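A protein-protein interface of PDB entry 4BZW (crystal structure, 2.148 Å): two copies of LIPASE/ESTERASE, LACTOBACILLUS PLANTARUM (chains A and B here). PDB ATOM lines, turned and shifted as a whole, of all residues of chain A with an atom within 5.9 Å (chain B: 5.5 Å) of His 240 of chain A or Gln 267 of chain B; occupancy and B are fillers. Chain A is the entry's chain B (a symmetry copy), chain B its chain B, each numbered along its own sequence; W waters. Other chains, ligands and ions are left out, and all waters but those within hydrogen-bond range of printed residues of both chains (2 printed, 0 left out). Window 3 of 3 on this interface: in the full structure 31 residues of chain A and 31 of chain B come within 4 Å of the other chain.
The backbone carbonyl oxygen (O) of Ala 63 of chain B sits close to a ring nitrogen (NE2) of His 240 of chain A, at 3.3 Å. N of His 240 of chain A lies within hydrogen-bond range of OD1 of Asn 275 of chain B (2.8 Å).
The guanidinium group (NE) of Arg 264 of chain B lies within hydrogen-bond range of the side-chain amide oxygen (OE1) of Gln 267 of chain B, at 3.4 Å. The backbone carbonyl oxygen (O) of Ala 273 of chain B lies within hydrogen-bond range of the side-chain amide nitrogen (NE2) of Gln 267 of chain B, at 3.0 Å. The side-chain amide nitrogen of Gln 267 of chain B lies close to the side-chain amide nitrogen of Asn 275 of chain B, 3.3 Å away. The side-chain amide oxygen of Asn 239 of chain A lies within hydrogen-bond range of the backbone NH of Val 241 of chain A, at 3.0 Å.
Among the printed residues, pairs that only touch across the chains: Asn 239 of chain A with Asn 275 of chain B (3.3 Å), His 240 of chain A with Gln 267 of chain B (3.8 Å), His 240 of chain A with Leu 272 of chain B (3.9 Å), His 240 of chain A with Ala 273 of chain B (3.3 Å), His 240 of chain A with Gly 274 of chain B (3.3 Å), Val 241 of chain A with Ala 63 of chain B (3.6 Å), Val 241 of chain A with Gly 64 of chain B (3.9 Å) and Leu 251 of chain A with Asn 275 of chain B (3.9 Å).
His 240 of chain A touches just these residues of chain B: Ala 63, Gln 267, Leu 272, Ala 273, Gly 274 and Asn 275. Of the printed residues of chain A, Gln 267 of chain B touches His 240. Printed residues of chain A within 4 Å of Asn 275 of chain B: Asn 239 (3.3 Å), His 240 (2.8 Å) and Leu 251 (3.9 Å). Printed residues of chain A within 4 Å of Gly 64 of chain B: Val 241. Leu 271 of chain B touches none of the printed residues of chain A. The nearest printed residue of chain A that does not touch Gln 267 of chain B is Asn 239 of chain A (6.8 Å).
Hydrophobic or aromatic side chains of chain B within 4 Å of the printed part of chain A: Leu 272 and Ala 273. Of the 7 printed residues of chain A, 4 touch a printed residue of chain B. Hydrophobic or aromatic side chains of chain A that line the printed part of chain B: His 240, Val 241 and Leu 251. Among the printed residues, 10 pairs touch across the chains.
No position is printed for both chains.
Water W1 bridges the backbone carbonyl oxygen (O) of Gly 64 of chain B and a ring nitrogen (ND1) of His 240 of chain A. Water W2 lies within hydrogen-bond range of the side-chain amide oxygen of Gln 243 of chain A (2.6 Å) and the backbone carbonyl oxygen of Gly 274 of chain B (2.6 Å).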
ATOM      1  N   ALA A 238      13.851 -15.381  37.658  1.00  0.00           N
ATOM      2  CA  ALA A 238      12.796 -15.913  36.784  1.00  0.00           C
ATOM      3  C   ALA A 238      13.323 -16.854  35.697  1.00  0.00           C
ATOM      4  O   ALA A 238      12.681 -17.064  34.651  1.00  0.00           O
ATOM      5  CB  ALA A 238      11.965 -14.766  36.165  1.00  0.00           C
ATOM      6  N   ASN A 239      14.490 -17.438  35.949  1.00  0.00           N
ATOM      7  CA  ASN A 239      15.071 -18.365  34.991  1.00  0.00           C
ATOM      8  C   ASN A 239      15.624 -19.605  35.694  1.00  0.00           C
ATOM      9  O   ASN A 239      15.402 -19.791  36.897  1.00  0.00           O
ATOM     10  CB  ASN A 239      16.132 -17.660  34.125  1.00  0.00           C
ATOM     11  CG  ASN A 239      17.394 -17.274  34.913  1.00  0.00           C
ATOM     12  OD1 ASN A 239      17.579 -17.679  36.064  1.00  0.00           O
ATOM     13  ND2 ASN A 239      18.272 -16.497  34.283  1.00  0.00           N
ATOM     14  N   HIS A 240      16.346 -20.447  34.958  1.00  0.00           N
ATOM     15  CA  HIS A 240      16.795 -21.733  35.498  1.00  0.00           C
ATOM     16  C   HIS A 240      17.713 -21.600  36.721  1.00  0.00           C
ATOM     17  O   HIS A 240      17.767 -22.487  37.570  1.00  0.00           O
ATOM     18  CB  HIS A 240      17.496 -22.546  34.409  1.00  0.00           C
ATOM     19  CG  HIS A 240      18.809 -21.966  33.984  1.00  0.00           C
ATOM     20  ND1 HIS A 240      20.015 -22.408  34.485  1.00  0.00           N
ATOM     21  CD2 HIS A 240      19.105 -20.975  33.109  1.00  0.00           C
ATOM     22  CE1 HIS A 240      20.999 -21.722  33.930  1.00  0.00           C
ATOM     23  NE2 HIS A 240      20.473 -20.842  33.095  1.00  0.00           N
ATOM     24  N   VAL A 241      18.429 -20.487  36.809  1.00  0.00           N
ATOM     25  CA  VAL A 241      19.355 -20.252  37.910  1.00  0.00           C
ATOM     26  C   VAL A 241      18.652 -20.244  39.278  1.00  0.00           C
ATOM     27  O   VAL A 241      19.093 -20.915  40.217  1.00  0.00           O
ATOM     28  CB  VAL A 241      20.125 -18.925  37.696  1.00  0.00           C
ATOM     29  CG1 VAL A 241      21.140 -18.696  38.818  1.00  0.00           C
ATOM     30  CG2 VAL A 241      20.827 -18.940  36.326  1.00  0.00           C
ATOM     31  N   THR A 242      17.554 -19.504  39.393  1.00  0.00           N
ATOM     32  CA  THR A 242      16.862 -19.391  40.682  1.00  0.00           C
ATOM     33  C   THR A 242      15.634 -20.290  40.760  1.00  0.00           C
ATOM     34  O   THR A 242      14.827 -20.192  41.693  1.00  0.00           O
ATOM     35  CB  THR A 242      16.489 -17.921  41.004  1.00  0.00           C
ATOM     36  OG1 THR A 242      15.772 -17.354  39.898  1.00  0.00           O
ATOM     37  CG2 THR A 242      17.747 -17.114  41.230  1.00  0.00           C
ATOM     38  N   GLN A 243      15.504 -21.179  39.782  1.00  0.00           N
ATOM     39  CA  GLN A 243      14.363 -22.086  39.741  1.00  0.00           C
ATOM     40  C   GLN A 243      14.498 -23.211  40.760  1.00  0.00           C
ATOM     41  O   GLN A 243      15.488 -23.951  40.745  1.00  0.00           O
ATOM     42  CB  GLN A 243      14.213 -22.696  38.343  1.00  0.00           C
ATOM     43  CG  GLN A 243      13.161 -23.797  38.273  1.00  0.00           C
ATOM     44  CD  GLN A 243      13.224 -24.600  36.987  1.00  0.00           C
ATOM     45  OE1 GLN A 243      14.223 -24.559  36.265  1.00  0.00           O
ATOM     46  NE2 GLN A 243      12.150 -25.333  36.690  1.00  0.00           N
ATOM     47  N   LEU A 251       9.844 -20.291  36.449  1.00  0.00           N
ATOM     48  CA  LEU A 251      10.305 -19.801  35.148  1.00  0.00           C
ATOM     49  C   LEU A 251       9.252 -18.871  34.533  1.00  0.00           C
ATOM     50  O   LEU A 251       8.065 -19.211  34.486  1.00  0.00           O
ATOM     51  CB  LEU A 251      10.573 -20.972  34.195  1.00  0.00           C
ATOM     52  CG  LEU A 251      11.532 -22.072  34.665  1.00  0.00           C
ATOM     53  CD1 LEU A 251      11.548 -23.237  33.676  1.00  0.00           C
ATOM     54  CD2 LEU A 251      12.937 -21.514  34.863  1.00  0.00           C
ATOM     55  N   ALA B  63      24.951 -17.020  34.774  1.00  0.00           N
ATOM     56  CA  ALA B  63      24.061 -17.946  34.080  1.00  0.00           C
ATOM     57  C   ALA B  63      24.053 -19.314  34.757  1.00  0.00           C
ATOM     58  O   ALA B  63      23.515 -20.280  34.208  1.00  0.00           O
ATOM     59  CB  ALA B  63      24.481 -18.089  32.623  1.00  0.00           C
ATOM     60  N   GLY B  64      24.657 -19.406  35.939  1.00  0.00           N
ATOM     61  CA  GLY B  64      24.583 -20.633  36.722  1.00  0.00           C
ATOM     62  C   GLY B  64      25.643 -21.679  36.417  1.00  0.00           C
ATOM     63  O   GLY B  64      25.343 -22.877  36.284  1.00  0.00           O
ATOM     64  N   ALA B 262      25.976 -17.459  23.102  1.00  0.00           N
ATOM     65  CA  ALA B 262      26.748 -18.629  23.522  1.00  0.00           C
ATOM     66  C   ALA B 262      26.000 -19.449  24.570  1.00  0.00           C
ATOM     67  O   ALA B 262      25.984 -20.682  24.516  1.00  0.00           O
ATOM     68  CB  ALA B 262      28.135 -18.213  24.048  1.00  0.00           C
ATOM     69  N   LEU B 263      25.389 -18.762  25.524  1.00  0.00           N
ATOM     70  CA  LEU B 263      24.614 -19.418  26.576  1.00  0.00           C
ATOM     71  C   LEU B 263      23.401 -20.176  26.017  1.00  0.00           C
ATOM     72  O   LEU B 263      23.118 -21.310  26.428  1.00  0.00           O
ATOM     73  CB  LEU B 263      24.165 -18.384  27.621  1.00  0.00           C
ATOM     74  CG  LEU B 263      25.313 -17.759  28.424  1.00  0.00           C
ATOM     75  CD1 LEU B 263      24.825 -16.555  29.229  1.00  0.00           C
ATOM     76  CD2 LEU B 263      25.974 -18.788  29.344  1.00  0.00           C
ATOM     77  N   ARG B 264      22.679 -19.545  25.095  1.00  0.00           N
ATOM     78  CA  ARG B 264      21.543 -20.188  24.441  1.00  0.00           C
ATOM     79  C   ARG B 264      22.009 -21.395  23.604  1.00  0.00           C
ATOM     80  O   ARG B 264      21.319 -22.415  23.513  1.00  0.00           O
ATOM     81  CB  ARG B 264      20.809 -19.169  23.562  1.00  0.00           C
ATOM     82  CG  ARG B 264      19.649 -19.747  22.759  1.00  0.00           C
ATOM     83  CD  ARG B 264      18.442 -20.108  23.637  1.00  0.00           C
ATOM     84  NE  ARG B 264      18.358 -21.546  23.898  1.00  0.00           N
ATOM     85  CZ  ARG B 264      17.626 -22.398  23.187  1.00  0.00           C
ATOM     86  NH1 ARG B 264      16.902 -21.964  22.166  1.00  0.00           N
ATOM     87  NH2 ARG B 264      17.615 -23.690  23.499  1.00  0.00           N
ATOM     88  N   TRP B 265      23.182 -21.281  22.995  1.00  0.00           N
ATOM     89  CA  TRP B 265      23.755 -22.413  22.264  1.00  0.00           C
ATOM     90  C   TRP B 265      24.094 -23.578  23.216  1.00  0.00           C
ATOM     91  O   TRP B 265      23.831 -24.744  22.906  1.00  0.00           O
ATOM     92  CB  TRP B 265      24.995 -21.964  21.492  1.00  0.00           C
ATOM     93  CG  TRP B 265      25.696 -23.058  20.721  1.00  0.00           C
ATOM     94  CD1 TRP B 265      25.374 -23.532  19.471  1.00  0.00           C
ATOM     95  CD2 TRP B 265      26.858 -23.786  21.139  1.00  0.00           C
ATOM     96  NE1 TRP B 265      26.270 -24.516  19.096  1.00  0.00           N
ATOM     97  CE2 TRP B 265      27.188 -24.688  20.101  1.00  0.00           C
ATOM     98  CE3 TRP B 265      27.652 -23.763  22.292  1.00  0.00           C
ATOM     99  CZ2 TRP B 265      28.280 -25.566  20.188  1.00  0.00           C
ATOM    100  CZ3 TRP B 265      28.735 -24.630  22.379  1.00  0.00           C
ATOM    101  CH2 TRP B 265      29.039 -25.522  21.331  1.00  0.00           C
ATOM    102  N   LEU B 266      24.664 -23.262  24.377  1.00  0.00           N
ATOM    103  CA  LEU B 266      24.959 -24.298  25.371  1.00  0.00           C
ATOM    104  C   LEU B 266      23.685 -25.017  25.809  1.00  0.00           C
ATOM    105  O   LEU B 266      23.681 -26.243  25.984  1.00  0.00           O
ATOM    106  CB  LEU B 266      25.673 -23.708  26.591  1.00  0.00           C
ATOM    107  CG  LEU B 266      27.150 -23.338  26.451  1.00  0.00           C
ATOM    108  CD1 LEU B 266      27.614 -22.589  27.699  1.00  0.00           C
ATOM    109  CD2 LEU B 266      28.018 -24.578  26.212  1.00  0.00           C
ATOM    110  N   GLN B 267      22.605 -24.257  25.985  1.00  0.00           N
ATOM    111  CA  GLN B 267      21.329 -24.846  26.392  1.00  0.00           C
ATOM    112  C   GLN B 267      20.839 -25.814  25.317  1.00  0.00           C
ATOM    113  O   GLN B 267      20.387 -26.920  25.621  1.00  0.00           O
ATOM    114  CB  GLN B 267      20.290 -23.753  26.680  1.00  0.00           C
ATOM    115  CG  GLN B 267      20.530 -23.000  27.994  1.00  0.00           C
ATOM    116  CD  GLN B 267      19.664 -21.759  28.123  1.00  0.00           C
ATOM    117  OE1 GLN B 267      19.424 -21.064  27.136  1.00  0.00           O
ATOM    118  NE2 GLN B 267      19.186 -21.476  29.342  1.00  0.00           N
ATOM    119  N   GLU B 268      20.962 -25.399  24.062  1.00  0.00           N
ATOM    120  CA  GLU B 268      20.585 -26.232  22.925  1.00  0.00           C
ATOM    121  C   GLU B 268      21.399 -27.530  22.872  1.00  0.00           C
ATOM    122  O   GLU B 268      20.895 -28.579  22.463  1.00  0.00           O
ATOM    123  CB  GLU B 268      20.756 -25.444  21.616  1.00  0.00           C
ATOM    124  CG  GLU B 268      20.721 -26.302  20.366  1.00  0.00           C
ATOM    125  CD  GLU B 268      20.566 -25.482  19.099  1.00  0.00           C
ATOM    126  OE1 GLU B 268      21.565 -24.866  18.655  1.00  0.00           O
ATOM    127  OE2 GLU B 268      19.440 -25.458  18.552  1.00  0.00           O
ATOM    128  N   GLN B 269      22.658 -27.455  23.288  1.00  0.00           N
ATOM    129  CA  GLN B 269      23.520 -28.631  23.298  1.00  0.00           C
ATOM    130  C   GLN B 269      23.203 -29.539  24.483  1.00  0.00           C
ATOM    131  O   GLN B 269      23.750 -30.634  24.590  1.00  0.00           O
ATOM    132  CB  GLN B 269      24.991 -28.209  23.338  1.00  0.00           C
ATOM    133  CG  GLN B 269      25.495 -27.570  22.041  1.00  0.00           C
ATOM    134  CD  GLN B 269      25.439 -28.524  20.861  1.00  0.00           C
ATOM    135  OE1 GLN B 269      24.857 -28.215  19.819  1.00  0.00           O
ATOM    136  NE2 GLN B 269      26.051 -29.694  21.019  1.00  0.00           N
ATOM    137  N   GLY B 270      22.321 -29.080  25.368  1.00  0.00           N
ATOM    138  CA  GLY B 270      21.991 -29.823  26.574  1.00  0.00           C
ATOM    139  C   GLY B 270      23.067 -29.719  27.648  1.00  0.00           C
ATOM    140  O   GLY B 270      23.155 -30.577  28.532  1.00  0.00           O
ATOM    141  N   LEU B 271      23.876 -28.662  27.575  1.00  0.00           N
ATOM    142  CA  LEU B 271      25.029 -28.482  28.458  1.00  0.00           C
ATOM    143  C   LEU B 271      24.802 -27.418  29.535  1.00  0.00           C
ATOM    144  O   LEU B 271      25.679 -27.157  30.365  1.00  0.00           O
ATOM    145  CB  LEU B 271      26.268 -28.135  27.629  1.00  0.00           C
ATOM    146  CG  LEU B 271      26.671 -29.219  26.632  1.00  0.00           C
ATOM    147  CD1 LEU B 271      27.870 -28.774  25.837  1.00  0.00           C
ATOM    148  CD2 LEU B 271      26.955 -30.539  27.346  1.00  0.00           C
ATOM    149  N   LEU B 272      23.621 -26.809  29.514  1.00  0.00           N
ATOM    150  CA  LEU B 272      23.239 -25.793  30.492  1.00  0.00           C
ATOM    151  C   LEU B 272      21.730 -25.906  30.657  1.00  0.00           C
ATOM    152  O   LEU B 272      21.021 -26.048  29.659  1.00  0.00           O
ATOM    153  CB  LEU B 272      23.585 -24.403  29.965  1.00  0.00           C
ATOM    154  CG  LEU B 272      23.279 -23.206  30.868  1.00  0.00           C
ATOM    155  CD1 LEU B 272      24.104 -23.282  32.145  1.00  0.00           C
ATOM    156  CD2 LEU B 272      23.551 -21.912  30.127  1.00  0.00           C
ATOM    157  N   ALA B 273      21.229 -25.852  31.891  1.00  0.00           N
ATOM    158  CA  ALA B 273      19.782 -25.988  32.114  1.00  0.00           C
ATOM    159  C   ALA B 273      19.002 -24.912  31.362  1.00  0.00           C
ATOM    160  O   ALA B 273      19.455 -23.768  31.251  1.00  0.00           O
ATOM    161  CB  ALA B 273      19.442 -25.962  33.602  1.00  0.00           C
ATOM    162  N   GLY B 274      17.839 -25.286  30.836  1.00  0.00           N
ATOM    163  CA  GLY B 274      17.062 -24.404  29.981  1.00  0.00           C
ATOM    164  C   GLY B 274      15.981 -23.648  30.727  1.00  0.00           C
ATOM    165  O   GLY B 274      15.772 -23.857  31.924  1.00  0.00           O
ATOM    166  N   ASN B 275      15.281 -22.775  30.008  1.00  0.00           N
ATOM    167  CA  ASN B 275      14.279 -21.899  30.613  1.00  0.00           C
ATOM    168  C   ASN B 275      12.849 -22.176  30.139  1.00  0.00           C
ATOM    169  O   ASN B 275      11.953 -21.346  30.313  1.00  0.00           O
ATOM    170  CB  ASN B 275      14.656 -20.432  30.370  1.00  0.00           C
ATOM    171  CG  ASN B 275      15.958 -20.049  31.053  1.00  0.00           C
ATOM    172  OD1 ASN B 275      16.176 -20.385  32.213  1.00  0.00           O
ATOM    173  ND2 ASN B 275      16.831 -19.357  30.334  1.00  0.00           N
HETATM  174  O   HOH W   1      22.988 -23.723  35.596  1.00  0.00           O
HETATM  175  O   HOH W   2      14.968 -25.370  33.897  1.00  0.00           O
